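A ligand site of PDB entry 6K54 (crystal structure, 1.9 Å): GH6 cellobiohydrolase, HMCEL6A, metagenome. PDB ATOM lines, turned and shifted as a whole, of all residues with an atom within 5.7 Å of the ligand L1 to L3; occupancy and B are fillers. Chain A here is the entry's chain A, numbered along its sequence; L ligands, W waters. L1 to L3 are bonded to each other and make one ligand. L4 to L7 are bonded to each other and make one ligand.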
ATOM      1  N   TYR A  86      13.726 -11.329  11.416  1.00  0.00           N
ATOM      2  CA  TYR A  86      12.751 -12.289  11.969  1.00  0.00           C
ATOM      3  C   TYR A  86      11.346 -12.004  11.422  1.00  0.00           C
ATOM      4  O   TYR A  86      10.439 -11.589  12.155  1.00  0.00           O
ATOM      5  CB  TYR A  86      12.767 -12.238  13.487  1.00  0.00           C
ATOM      6  CG  TYR A  86      11.951 -13.309  14.184  1.00  0.00           C
ATOM      7  CD1 TYR A  86      12.177 -14.663  13.935  1.00  0.00           C
ATOM      8  CD2 TYR A  86      10.965 -12.972  15.100  1.00  0.00           C
ATOM      9  CE1 TYR A  86      11.435 -15.646  14.586  1.00  0.00           C
ATOM     10  CE2 TYR A  86      10.211 -13.940  15.745  1.00  0.00           C
ATOM     11  CZ  TYR A  86      10.448 -15.272  15.498  1.00  0.00           C
ATOM     12  OH  TYR A  86       9.695 -16.240  16.143  1.00  0.00           O
ATOM     13  N   ASP A  92       7.591 -19.153  12.745  1.00  0.00           N
ATOM     14  CA  ASP A  92       7.316 -19.921  13.957  1.00  0.00           C
ATOM     15  C   ASP A  92       6.439 -21.124  13.643  1.00  0.00           C
ATOM     16  O   ASP A  92       5.475 -21.423  14.361  1.00  0.00           O
ATOM     17  CB  ASP A  92       6.687 -19.032  15.037  1.00  0.00           C
ATOM     18  CG  ASP A  92       6.863 -19.595  16.452  1.00  0.00           C
ATOM     19  OD1 ASP A  92       7.847 -20.355  16.685  1.00  0.00           O
ATOM     20  OD2 ASP A  92       6.033 -19.262  17.331  1.00  0.00           O
ATOM     21  N   SER A  94       6.262 -24.266  13.785  1.00  0.00           N
ATOM     22  CA  SER A  94       5.967 -25.364  14.696  1.00  0.00           C
ATOM     23  C   SER A  94       5.315 -24.944  16.020  1.00  0.00           C
ATOM     24  O   SER A  94       5.145 -25.793  16.899  1.00  0.00           O
ATOM     25  CB  SER A  94       7.240 -26.189  14.914  1.00  0.00           C
ATOM     26  OG  SER A  94       8.133 -25.597  15.832  1.00  0.00           O
ATOM     27  N   ALA A  95       4.912 -23.680  16.175  1.00  0.00           N
ATOM     28  CA  ALA A  95       4.270 -23.247  17.415  1.00  0.00           C
ATOM     29  C   ALA A  95       3.259 -22.153  17.088  1.00  0.00           C
ATOM     30  O   ALA A  95       3.011 -21.830  15.926  1.00  0.00           O
ATOM     31  CB  ALA A  95       5.322 -22.771  18.434  1.00  0.00           C
ATOM     32  N   SER A  98       4.496 -17.120  18.326  1.00  0.00           N
ATOM     33  CA  SER A  98       5.177 -16.075  17.552  1.00  0.00           C
ATOM     34  C   SER A  98       4.911 -16.174  16.049  1.00  0.00           C
ATOM     35  O   SER A  98       5.744 -15.774  15.239  1.00  0.00           O
ATOM     36  CB  SER A  98       6.687 -16.094  17.813  1.00  0.00           C
ATOM     37  OG  SER A  98       6.980 -15.624  19.114  1.00  0.00           O
ATOM     38  N   ASP A 141      14.876 -20.232  14.310  1.00  0.00           N
ATOM     39  CA  ASP A 141      13.928 -21.364  14.344  1.00  0.00           C
ATOM     40  C   ASP A 141      13.549 -21.892  12.959  1.00  0.00           C
ATOM     41  O   ASP A 141      13.128 -23.057  12.846  1.00  0.00           O
ATOM     42  CB  ASP A 141      12.643 -21.027  15.092  1.00  0.00           C
ATOM     43  CG  ASP A 141      12.895 -20.595  16.539  1.00  0.00           C
ATOM     44  OD1 ASP A 141      13.933 -20.996  17.114  1.00  0.00           O
ATOM     45  OD2 ASP A 141      12.048 -19.831  17.083  1.00  0.00           O
ATOM     46  N   ASN A 145      13.321 -25.964  12.198  1.00  0.00           N
ATOM     47  CA  ASN A 145      11.999 -26.546  11.975  1.00  0.00           C
ATOM     48  C   ASN A 145      11.957 -27.436  10.728  1.00  0.00           C
ATOM     49  O   ASN A 145      11.199 -28.415  10.692  1.00  0.00           O
ATOM     50  CB  ASN A 145      10.950 -25.449  11.895  1.00  0.00           C
ATOM     51  CG  ASN A 145      10.423 -25.080  13.252  1.00  0.00           C
ATOM     52  OD1 ASN A 145      10.283 -25.934  14.128  1.00  0.00           O
ATOM     53  ND2 ASN A 145      10.142 -23.789  13.445  1.00  0.00           N
ATOM     54  N   THR A 148      13.249 -30.994  11.888  1.00  0.00           N
ATOM     55  CA  THR A 148      12.501 -31.833  12.816  1.00  0.00           C
ATOM     56  C   THR A 148      10.990 -31.778  12.648  1.00  0.00           C
ATOM     57  O   THR A 148      10.298 -32.646  13.199  1.00  0.00           O
ATOM     58  CB  THR A 148      12.835 -31.465  14.279  1.00  0.00           C
ATOM     59  OG1 THR A 148      12.341 -30.146  14.576  1.00  0.00           O
ATOM     60  CG2 THR A 148      14.354 -31.500  14.517  1.00  0.00           C
ATOM     61  N   ASN A 149      10.439 -30.819  11.912  1.00  0.00           N
ATOM     62  CA  ASN A 149       9.004 -30.584  11.955  1.00  0.00           C
ATOM     63  C   ASN A 149       8.348 -30.649  10.574  1.00  0.00           C
ATOM     64  O   ASN A 149       7.333 -30.002  10.347  1.00  0.00           O
ATOM     65  CB  ASN A 149       8.701 -29.240  12.620  1.00  0.00           C
ATOM     66  CG  ASN A 149       8.750 -29.347  14.137  1.00  0.00           C
ATOM     67  OD1 ASN A 149       8.156 -30.265  14.709  1.00  0.00           O
ATOM     68  ND2 ASN A 149       9.457 -28.420  14.798  1.00  0.00           N
ATOM     69  N   HIS A 187      19.566 -25.263  19.289  1.00  0.00           N
ATOM     70  CA  HIS A 187      20.334 -25.493  20.504  1.00  0.00           C
ATOM     71  C   HIS A 187      20.450 -26.993  20.683  1.00  0.00           C
ATOM     72  O   HIS A 187      19.817 -27.771  19.967  1.00  0.00           O
ATOM     73  CB  HIS A 187      19.670 -24.846  21.731  1.00  0.00           C
ATOM     74  CG  HIS A 187      18.290 -25.360  22.023  1.00  0.00           C
ATOM     75  ND1 HIS A 187      18.031 -26.307  22.984  1.00  0.00           N
ATOM     76  CD2 HIS A 187      17.094 -25.039  21.472  1.00  0.00           C
ATOM     77  CE1 HIS A 187      16.736 -26.562  23.011  1.00  0.00           C
ATOM     78  NE2 HIS A 187      16.149 -25.799  22.111  1.00  0.00           N
ATOM     79  N   GLY A 189      19.434 -29.053  22.889  1.00  0.00           N
ATOM     80  CA  GLY A 189      18.199 -29.728  23.226  1.00  0.00           C
ATOM     81  C   GLY A 189      17.174 -29.751  22.115  1.00  0.00           C
ATOM     82  O   GLY A 189      16.018 -30.107  22.355  1.00  0.00           O
ATOM     83  N   TRP A 190      17.575 -29.356  20.911  1.00  0.00           N
ATOM     84  CA  TRP A 190      16.740 -29.445  19.706  1.00  0.00           C
ATOM     85  C   TRP A 190      17.405 -30.333  18.661  1.00  0.00           C
ATOM     86  O   TRP A 190      16.799 -31.316  18.231  1.00  0.00           O
ATOM     87  CB  TRP A 190      16.462 -28.036  19.137  1.00  0.00           C
ATOM     88  CG  TRP A 190      15.394 -27.926  18.011  1.00  0.00           C
ATOM     89  CD1 TRP A 190      14.917 -28.932  17.220  1.00  0.00           C
ATOM     90  CD2 TRP A 190      14.720 -26.729  17.582  1.00  0.00           C
ATOM     91  NE1 TRP A 190      13.981 -28.448  16.331  1.00  0.00           N
ATOM     92  CE2 TRP A 190      13.843 -27.099  16.535  1.00  0.00           C
ATOM     93  CE3 TRP A 190      14.776 -25.389  17.994  1.00  0.00           C
ATOM     94  CZ2 TRP A 190      13.026 -26.162  15.879  1.00  0.00           C
ATOM     95  CZ3 TRP A 190      13.964 -24.459  17.342  1.00  0.00           C
ATOM     96  CH2 TRP A 190      13.092 -24.847  16.307  1.00  0.00           C
ATOM     97  N   TRP A 193      20.552 -34.782  18.950  1.00  0.00           N
ATOM     98  CA  TRP A 193      20.455 -36.185  18.552  1.00  0.00           C
ATOM     99  C   TRP A 193      21.118 -36.415  17.195  1.00  0.00           C
ATOM    100  O   TRP A 193      21.045 -35.556  16.302  1.00  0.00           O
ATOM    101  CB  TRP A 193      18.998 -36.648  18.490  1.00  0.00           C
ATOM    102  CG  TRP A 193      18.287 -36.681  19.835  1.00  0.00           C
ATOM    103  CD1 TRP A 193      18.203 -37.737  20.689  1.00  0.00           C
ATOM    104  CD2 TRP A 193      17.552 -35.604  20.436  1.00  0.00           C
ATOM    105  NE1 TRP A 193      17.464 -37.388  21.799  1.00  0.00           N
ATOM    106  CE2 TRP A 193      17.061 -36.078  21.672  1.00  0.00           C
ATOM    107  CE3 TRP A 193      17.274 -34.286  20.064  1.00  0.00           C
ATOM    108  CZ2 TRP A 193      16.296 -35.289  22.524  1.00  0.00           C
ATOM    109  CZ3 TRP A 193      16.509 -33.497  20.916  1.00  0.00           C
ATOM    110  CH2 TRP A 193      16.044 -33.996  22.141  1.00  0.00           C
ATOM    111  N   ASN A 196      19.101 -35.596  14.028  1.00  0.00           N
ATOM    112  CA  ASN A 196      18.867 -34.159  13.873  1.00  0.00           C
ATOM    113  C   ASN A 196      20.166 -33.413  13.562  1.00  0.00           C
ATOM    114  O   ASN A 196      20.172 -32.502  12.717  1.00  0.00           O
ATOM    115  CB  ASN A 196      18.245 -33.580  15.148  1.00  0.00           C
ATOM    116  CG  ASN A 196      16.841 -34.087  15.404  1.00  0.00           C
ATOM    117  OD1 ASN A 196      16.280 -34.827  14.613  1.00  0.00           O
ATOM    118  ND2 ASN A 196      16.279 -33.679  16.529  1.00  0.00           N
ATOM    119  N   VAL A 225      19.381 -19.268  20.701  1.00  0.00           N
ATOM    120  CA  VAL A 225      18.591 -18.044  20.620  1.00  0.00           C
ATOM    121  C   VAL A 225      17.265 -18.252  21.320  1.00  0.00           C
ATOM    122  O   VAL A 225      16.512 -19.189  21.020  1.00  0.00           O
ATOM    123  CB  VAL A 225      18.372 -17.620  19.165  1.00  0.00           C
ATOM    124  CG1 VAL A 225      17.373 -16.446  19.084  1.00  0.00           C
ATOM    125  CG2 VAL A 225      19.699 -17.263  18.510  1.00  0.00           C
ATOM    126  N   ALA A 226      16.978 -17.356  22.275  1.00  0.00           N
ATOM    127  CA  ALA A 226      15.750 -17.339  23.064  1.00  0.00           C
ATOM    128  C   ALA A 226      15.540 -18.615  23.860  1.00  0.00           C
ATOM    129  O   ALA A 226      14.426 -18.835  24.363  1.00  0.00           O
ATOM    130  CB  ALA A 226      14.524 -17.046  22.168  1.00  0.00           C
ATOM    131  N   ASN A 227      16.560 -19.470  24.015  1.00  0.00           N
ATOM    132  CA  ASN A 227      16.359 -20.646  24.850  1.00  0.00           C
ATOM    133  C   ASN A 227      17.195 -20.514  26.126  1.00  0.00           C
ATOM    134  O   ASN A 227      17.731 -19.453  26.455  1.00  0.00           O
ATOM    135  CB  ASN A 227      16.647 -21.931  24.062  1.00  0.00           C
ATOM    136  CG  ASN A 227      15.814 -23.118  24.567  1.00  0.00           C
ATOM    137  OD1 ASN A 227      15.983 -23.577  25.698  1.00  0.00           O
ATOM    138  ND2 ASN A 227      14.878 -23.580  23.731  1.00  0.00           N
ATOM    139  N   GLU A 255      17.356 -38.480  26.666  1.00  0.00           N
ATOM    140  CA  GLU A 255      16.873 -39.413  25.637  1.00  0.00           C
ATOM    141  C   GLU A 255      17.950 -39.754  24.609  1.00  0.00           C
ATOM    142  O   GLU A 255      17.712 -39.731  23.395  1.00  0.00           O
ATOM    143  CB  GLU A 255      15.618 -38.852  24.949  1.00  0.00           C
ATOM    144  CG  GLU A 255      14.491 -38.521  25.913  1.00  0.00           C
ATOM    145  CD  GLU A 255      13.295 -37.848  25.230  1.00  0.00           C
ATOM    146  OE1 GLU A 255      13.461 -36.775  24.598  1.00  0.00           O
ATOM    147  OE2 GLU A 255      12.179 -38.406  25.348  1.00  0.00           O
ATOM    148  N   HIS A 327      11.374 -30.670  31.531  1.00  0.00           N
ATOM    149  CA  HIS A 327      11.601 -31.365  30.272  1.00  0.00           C
ATOM    150  C   HIS A 327      12.399 -30.423  29.380  1.00  0.00           C
ATOM    151  O   HIS A 327      12.196 -29.208  29.399  1.00  0.00           O
ATOM    152  CB  HIS A 327      10.266 -31.774  29.625  1.00  0.00           C
ATOM    153  CG  HIS A 327      10.424 -32.602  28.388  1.00  0.00           C
ATOM    154  ND1 HIS A 327      10.605 -32.049  27.137  1.00  0.00           N
ATOM    155  CD2 HIS A 327      10.402 -33.944  28.204  1.00  0.00           C
ATOM    156  CE1 HIS A 327      10.706 -33.008  26.242  1.00  0.00           C
ATOM    157  NE2 HIS A 327      10.597 -34.176  26.857  1.00  0.00           N
ATOM    158  N   ARG A 328      13.328 -30.994  28.607  1.00  0.00           N
ATOM    159  CA  ARG A 328      14.241 -30.163  27.846  1.00  0.00           C
ATOM    160  C   ARG A 328      13.554 -29.353  26.755  1.00  0.00           C
ATOM    161  O   ARG A 328      14.107 -28.342  26.299  1.00  0.00           O
ATOM    162  CB  ARG A 328      15.332 -31.034  27.234  1.00  0.00           C
ATOM    163  CG  ARG A 328      16.676 -30.452  27.379  1.00  0.00           C
ATOM    164  CD  ARG A 328      17.775 -31.349  26.850  1.00  0.00           C
ATOM    165  NE  ARG A 328      18.998 -30.569  26.801  1.00  0.00           N
ATOM    166  CZ  ARG A 328      20.057 -30.868  26.078  1.00  0.00           C
ATOM    167  NH1 ARG A 328      20.052 -31.958  25.310  1.00  0.00           N
ATOM    168  NH2 ARG A 328      21.122 -30.076  26.122  1.00  0.00           N
ATOM    169  N   GLY A 329      12.369 -29.784  26.299  1.00  0.00           N
ATOM    170  CA  GLY A 329      11.603 -29.060  25.304  1.00  0.00           C
ATOM    171  C   GLY A 329      10.786 -27.900  25.839  1.00  0.00           C
ATOM    172  O   GLY A 329      10.099 -27.230  25.057  1.00  0.00           O
ATOM    173  N   ASN A 330      10.846 -27.627  27.143  1.00  0.00           N
ATOM    174  CA  ASN A 330      10.080 -26.531  27.749  1.00  0.00           C
ATOM    175  C   ASN A 330      10.713 -25.183  27.399  1.00  0.00           C
ATOM    176  O   ASN A 330      11.566 -24.685  28.154  1.00  0.00           O
ATOM    177  CB  ASN A 330       9.991 -26.700  29.272  1.00  0.00           C
ATOM    178  CG  ASN A 330       9.080 -27.858  29.698  1.00  0.00           C
ATOM    179  OD1 ASN A 330       8.391 -28.459  28.871  1.00  0.00           O
ATOM    180  ND2 ASN A 330       9.069 -28.144  31.007  1.00  0.00           N
ATOM    181  N   TRP A 331      10.298 -24.585  26.290  1.00  0.00           N
ATOM    182  CA  TRP A 331      10.930 -23.371  25.801  1.00  0.00           C
ATOM    183  C   TRP A 331      10.244 -22.085  26.244  1.00  0.00           C
ATOM    184  O   TRP A 331      10.769 -21.005  25.979  1.00  0.00           O
ATOM    185  CB  TRP A 331      11.021 -23.389  24.265  1.00  0.00           C
ATOM    186  CG  TRP A 331       9.697 -23.658  23.586  1.00  0.00           C
ATOM    187  CD1 TRP A 331       9.241 -24.857  23.122  1.00  0.00           C
ATOM    188  CD2 TRP A 331       8.669 -22.696  23.288  1.00  0.00           C
ATOM    189  NE1 TRP A 331       7.982 -24.706  22.560  1.00  0.00           N
ATOM    190  CE2 TRP A 331       7.614 -23.398  22.662  1.00  0.00           C
ATOM    191  CE3 TRP A 331       8.539 -21.321  23.508  1.00  0.00           C
ATOM    192  CZ2 TRP A 331       6.443 -22.749  22.234  1.00  0.00           C
ATOM    193  CZ3 TRP A 331       7.368 -20.682  23.090  1.00  0.00           C
ATOM    194  CH2 TRP A 331       6.336 -21.405  22.466  1.00  0.00           C
ATOM    195  N   ARG A 391       3.476 -30.312  25.424  1.00  0.00           N
ATOM    196  CA  ARG A 391       2.914 -31.035  24.286  1.00  0.00           C
ATOM    197  C   ARG A 391       3.961 -31.866  23.560  1.00  0.00           C
ATOM    198  O   ARG A 391       3.632 -32.524  22.576  1.00  0.00           O
ATOM    199  CB  ARG A 391       2.194 -30.068  23.323  1.00  0.00           C
ATOM    200  CG  ARG A 391       2.989 -28.879  22.797  1.00  0.00           C
ATOM    201  CD  ARG A 391       2.070 -27.924  21.981  1.00  0.00           C
ATOM    202  NE  ARG A 391       2.782 -26.755  21.427  1.00  0.00           N
ATOM    203  CZ  ARG A 391       3.629 -26.834  20.402  1.00  0.00           C
ATOM    204  NH1 ARG A 391       3.868 -28.016  19.837  1.00  0.00           N
ATOM    205  NH2 ARG A 391       4.232 -25.746  19.946  1.00  0.00           N
ATOM    206  N   TYR A 392       5.210 -31.865  24.032  1.00  0.00           N
ATOM    207  CA  TYR A 392       6.210 -32.782  23.503  1.00  0.00           C
ATOM    208  C   TYR A 392       6.299 -34.061  24.327  1.00  0.00           C
ATOM    209  O   TYR A 392       6.676 -35.117  23.789  1.00  0.00           O
ATOM    210  CB  TYR A 392       7.585 -32.095  23.428  1.00  0.00           C
ATOM    211  CG  TYR A 392       7.569 -30.795  22.622  1.00  0.00           C
ATOM    212  CD1 TYR A 392       7.324 -30.791  21.242  1.00  0.00           C
ATOM    213  CD2 TYR A 392       7.781 -29.569  23.245  1.00  0.00           C
ATOM    214  CE1 TYR A 392       7.283 -29.583  20.511  1.00  0.00           C
ATOM    215  CE2 TYR A 392       7.739 -28.371  22.525  1.00  0.00           C
ATOM    216  CZ  TYR A 392       7.492 -28.386  21.165  1.00  0.00           C
ATOM    217  OH  TYR A 392       7.469 -27.187  20.477  1.00  0.00           O
HETATM  218  C1  LIG L   1      12.634 -33.378  18.630  1.00  0.00           C
HETATM  219  C2  LIG L   1      13.170 -31.960  18.870  1.00  0.00           C
HETATM  220  C3  LIG L   1      12.550 -31.361  20.125  1.00  0.00           C
HETATM  221  C4  LIG L   1      12.720 -32.278  21.316  1.00  0.00           C
HETATM  222  C5  LIG L   1      11.979 -31.744  22.535  1.00  0.00           C
HETATM  223  C6  LIG L   1      12.799 -34.223  19.880  1.00  0.00           C
HETATM  224  O1  LIG L   1      12.199 -35.502  19.650  1.00  0.00           O
HETATM  225  O2  LIG L   1      13.350 -34.044  17.586  1.00  0.00           O
HETATM  226  O3  LIG L   1      12.856 -31.101  17.766  1.00  0.00           O
HETATM  227  O4  LIG L   1      13.174 -30.098  20.401  1.00  0.00           O
HETATM  228  O5  LIG L   1      12.202 -33.582  21.000  1.00  0.00           O
HETATM  229  O6  LIG L   1      11.959 -32.731  23.541  1.00  0.00           O
HETATM  230  C1  LG2 L   2      13.218 -27.873  21.095  1.00  0.00           C
HETATM  231  C2  LG2 L   2      12.402 -26.608  21.199  1.00  0.00           C
HETATM  232  C3  LG2 L   2      11.656 -26.309  19.885  1.00  0.00           C
HETATM  233  C4  LG2 L   2      10.884 -27.543  19.394  1.00  0.00           C
HETATM  234  C5  LG2 L   2      10.234 -27.322  18.035  1.00  0.00           C
HETATM  235  C6  LG2 L   2      12.344 -29.016  20.564  1.00  0.00           C
HETATM  236  O1  LG2 L   2      13.740 -28.226  22.394  1.00  0.00           O
HETATM  237  O2  LG2 L   2      13.302 -25.547  21.506  1.00  0.00           O
HETATM  238  O3  LG2 L   2      10.689 -25.288  20.083  1.00  0.00           O
HETATM  239  O4  LG2 L   2      11.758 -28.669  19.303  1.00  0.00           O
HETATM  240  O5  LG2 L   2       9.456 -28.495  17.711  1.00  0.00           O
HETATM  241  C1  LG3 L   3       9.723 -23.214  19.544  1.00  0.00           C
HETATM  242  C2  LG3 L   3      10.068 -21.781  19.188  1.00  0.00           C
HETATM  243  C3  LG3 L   3      11.120 -21.248  20.154  1.00  0.00           C
HETATM  244  C4  LG3 L   3      12.333 -22.178  20.186  1.00  0.00           C
HETATM  245  C5  LG3 L   3      13.373 -21.710  21.206  1.00  0.00           C
HETATM  246  C6  LG3 L   3      10.996 -24.047  19.578  1.00  0.00           C
HETATM  247  O1  LG3 L   3       8.829 -23.750  18.572  1.00  0.00           O
HETATM  248  O2  LG3 L   3       8.854 -21.035  19.254  1.00  0.00           O
HETATM  249  O3  LG3 L   3      11.574 -19.963  19.716  1.00  0.00           O
HETATM  250  O4  LG3 L   3      11.903 -23.483  20.529  1.00  0.00           O
HETATM  251  O5  LG3 L   3      14.527 -22.555  21.138  1.00  0.00           O
HETATM  252  C1  LG4 L   4       9.282 -18.235  20.748  1.00  0.00           C
HETATM  253  C2  LG4 L   4      10.419 -17.802  21.665  1.00  0.00           C
HETATM  254  C3  LG4 L   4      10.131 -16.330  21.865  1.00  0.00           C
HETATM  255  C4  LG4 L   4      10.436 -15.664  20.538  1.00  0.00           C
HETATM  256  C5  LG4 L   4      10.222 -16.535  19.261  1.00  0.00           C
HETATM  257  C6  LG4 L   4      11.510 -16.580  18.422  1.00  0.00           C
HETATM  258  O1  LG4 L   4       8.037 -17.543  21.064  1.00  0.00           O
HETATM  259  O2  LG4 L   4      10.400 -18.473  22.907  1.00  0.00           O
HETATM  260  O3  LG4 L   4      10.879 -15.761  22.962  1.00  0.00           O
HETATM  261  O4  LG4 L   4       9.570 -14.548  20.523  1.00  0.00           O
HETATM  262  O5  LG4 L   4       9.768 -17.882  19.443  1.00  0.00           O
HETATM  263  O6  LG4 L   4      12.690 -17.010  19.121  1.00  0.00           O
HETATM  264  C1  LG5 L   5       9.020 -12.652  19.647  1.00  0.00           C
HETATM  265  C2  LG5 L   5       9.440 -11.288  19.144  1.00  0.00           C
HETATM  266  C3  LG5 L   5      10.408 -10.659  20.144  1.00  0.00           C
HETATM  267  C4  LG5 L   5      11.579 -11.605  20.413  1.00  0.00           C
HETATM  268  C5  LG5 L   5      12.442 -11.038  21.520  1.00  0.00           C
HETATM  269  C6  LG5 L   5      10.235 -13.514  19.912  1.00  0.00           C
HETATM  270  O1  LG5 L   5       8.218 -13.328  18.677  1.00  0.00           O
HETATM  271  O2  LG5 L   5       8.285 -10.450  18.998  1.00  0.00           O
HETATM  272  O3  LG5 L   5      10.897  -9.418  19.627  1.00  0.00           O
HETATM  273  O4  LG5 L   5      11.101 -12.869  20.849  1.00  0.00           O
HETATM  274  O5  LG5 L   5      11.592 -10.812  22.658  1.00  0.00           O
HETATM  275  C1  LG6 L   6      11.286  -7.125  20.342  1.00  0.00           C
HETATM  276  C2  LG6 L   6      10.671  -5.914  21.055  1.00  0.00           C
HETATM  277  C3  LG6 L   6       9.224  -5.705  20.628  1.00  0.00           C
HETATM  278  C4  LG6 L   6       8.444  -7.011  20.796  1.00  0.00           C
HETATM  279  C5  LG6 L   6       6.984  -6.881  20.390  1.00  0.00           C
HETATM  280  C6  LG6 L   6      10.386  -8.363  20.347  1.00  0.00           C
HETATM  281  O1  LG6 L   6      12.520  -7.467  20.964  1.00  0.00           O
HETATM  282  O2  LG6 L   6      11.424  -4.745  20.722  1.00  0.00           O
HETATM  283  O3  LG6 L   6       8.669  -4.688  21.465  1.00  0.00           O
HETATM  284  O4  LG6 L   6       9.036  -8.017  19.983  1.00  0.00           O
HETATM  285  O5  LG6 L   6       6.954  -6.494  19.017  1.00  0.00           O
HETATM  286  C1  LG7 L   7       7.051  -2.948  21.927  1.00  0.00           C
HETATM  287  C2  LG7 L   7       6.369  -1.745  21.294  1.00  0.00           C
HETATM  288  C3  LG7 L   7       7.403  -0.786  20.728  1.00  0.00           C
HETATM  289  C4  LG7 L   7       8.321  -1.532  19.766  1.00  0.00           C
HETATM  290  C5  LG7 L   7       9.360  -0.608  19.136  1.00  0.00           C
HETATM  291  C6  LG7 L   7       8.049  -3.575  20.949  1.00  0.00           C
HETATM  292  O1  LG7 L   7       6.074  -3.929  22.329  1.00  0.00           O
HETATM  293  O2  LG7 L   7       5.577  -1.064  22.285  1.00  0.00           O
HETATM  294  O3  LG7 L   7       6.764   0.286  20.014  1.00  0.00           O
HETATM  295  O4  LG7 L   7       8.972  -2.614  20.433  1.00  0.00           O
HETATM  296  O5  LG7 L   7       9.811  -1.212  17.919  1.00  0.00           O
HETATM  297  O   HOH W   1      13.590 -26.131  24.608  1.00  0.00           O
HETATM  298  O   HOH W   2      11.701 -34.864  15.692  1.00  0.00           O
HETATM  299  O   HOH W   3       6.563 -30.040  17.170  1.00  0.00           O
HETATM  300  O   HOH W   4       8.485 -22.795  15.725  1.00  0.00           O
HETATM  301  O   HOH W   5      16.799 -21.724  19.913  1.00  0.00           O
HETATM  302  O   HOH W   6      14.752 -31.597  24.188  1.00  0.00           O
HETATM  303  O   HOH W   7      11.037 -35.249  23.353  1.00  0.00           O
HETATM  304  O   HOH W   8      12.327 -37.142  21.863  1.00  0.00           O
HETATM  305  O   HOH W   9      10.602 -30.855  16.732  1.00  0.00           O
HETATM  306  O   HOH W  10       6.555 -19.664  19.892  1.00  0.00           O
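N of Ser 98 is in hydrogen-bond range of OD2 of Asp 92 (2.8 Å). The side-chain amide nitrogen of Asn 149 lies within hydrogen-bond range of the side-chain amide oxygen of Asn 145. A ring nitrogen (ND1) of His 187 is in hydrogen-bond range of the backbone NH of Gly 189 (3.1 Å). ND2 of Asn 330 lies close to N of His 327 (3.5 Å). The indole nitrogen (NE1) of Trp 190 sits at hydrogen-bond distance from the side-chain hydroxyl (OG1) of Thr 148, at 2.9 Å. OG of Ser 94 lies within hydrogen-bond range of OD1 of Asn 145. NE1 of Trp 331 lies within hydrogen-bond range of OH of Tyr 392 (3.3 Å). O of Glu 255 lies within hydrogen-bond range of NE1 of Trp 193.
Water W5 bridges an oxygen (O5) of LG3 L3 (2.7 Å) and the backbone carbonyl oxygen (O) of Val 225 (2.8 Å). Water W10 lies within hydrogen-bond range of the side-chain carboxylate (OD2) of Asp 92, an oxygen (O2) of LG3 L3 and an oxygen (O1) of LG4 L4. Water W8 bridges O1 of LIG L1 and OE1 of Glu 255. Water W4 lies within hydrogen-bond range of the side-chain carboxylate (OD1) of Asp 92 (2.7 Å), the side-chain hydroxyl (OG) of Ser 94 (2.8 Å), the side-chain amide nitrogen (ND2) of Asn 145 (3.0 Å) and an oxygen (O1) of LG3 L3 (3.0 Å). Water W6 bridges O of Gly 189 (2.7 Å) and O6 of LIG L1 (3.1 Å). Water W3 lies within hydrogen-bond range of OD1 of Asn 149 (2.9 Å) and O5 of LG2 L2 (3.3 Å).
O3 of LG3 L3 is in hydrogen-bond range of O5 of LG4 L4 (2.8 Å).
An oxygen (O3) of LG3 L3 lies within hydrogen-bond range of the side-chain carboxylate (OD2) of Asp 141. The side-chain amide nitrogen (ND2) of Asn 227 is in hydrogen-bond range of an oxygen (O5) of LG3 L3 (2.8 Å). The side-chain carboxylate (OD1) of Asp 92 lies within hydrogen-bond range of an oxygen (O2) of LG3 L3 (2.8 Å). The side-chain amide nitrogen (ND2) of Asn 149 is in hydrogen-bond range of an oxygen (O5) of LG2 L2 (2.9 Å). A ring nitrogen (NE2) of His 187 sits at hydrogen-bond distance from an oxygen (O2) of LG2 L2. O of Gly 189 is in hydrogen-bond range of O1 of LG2 L2, at 3.0 Å. The indole nitrogen (NE1) of Trp 190 sits close to an oxygen (O3) of LIG L1. ND2 of Asn 196 is in hydrogen-bond range of O2 of LIG L1, at 3.1 Å. An oxygen (O3) of LIG L1 sits at hydrogen-bond distance from the side-chain hydroxyl (OG1) of Thr 148 (3.4 Å). The side-chain hydroxyl (OG) of Ser 94 is in hydrogen-bond range of an oxygen (O1) of LG3 L3 (3.4 Å). The side-chain hydroxyl (OG) of Ser 98 sits at hydrogen-bond distance from an oxygen (O1) of LG5 L5 (2.6 Å).
CB of Ala 95 touches O1 of LG3 L3, at 3.6 Å. CH2 of Trp 193 touches C4 of LIG L1 (3.8 Å). Val 225 touches the ligand L1 to L3. CE1 of His 327 touches O6 of LIG L1, at 3.0 Å. Arg 328 touches the ligand L1 to L3. Gly 329 touches the ligand L1 to L3. CD1 of Trp 331 touches O3 of LG2 L2 (3.4 Å). OH of Tyr 392 touches C4 of LG2 L2, 3.6 Å away. 18 residues have an atom within 4 Å of the ligand L1 to L3: Asp 92, Ser 94, Ala 95, Asp 141, Thr 148, Asn 149, His 187, Gly 189, Trp 190, Trp 193, Asn 196, Val 225, Asn 227, His 327, Arg 328, Gly 329, Trp 331 and Tyr 392. The nearest printed residue that does not touch the ligand L1 to L3 is Asn 145 (4.1 Å).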
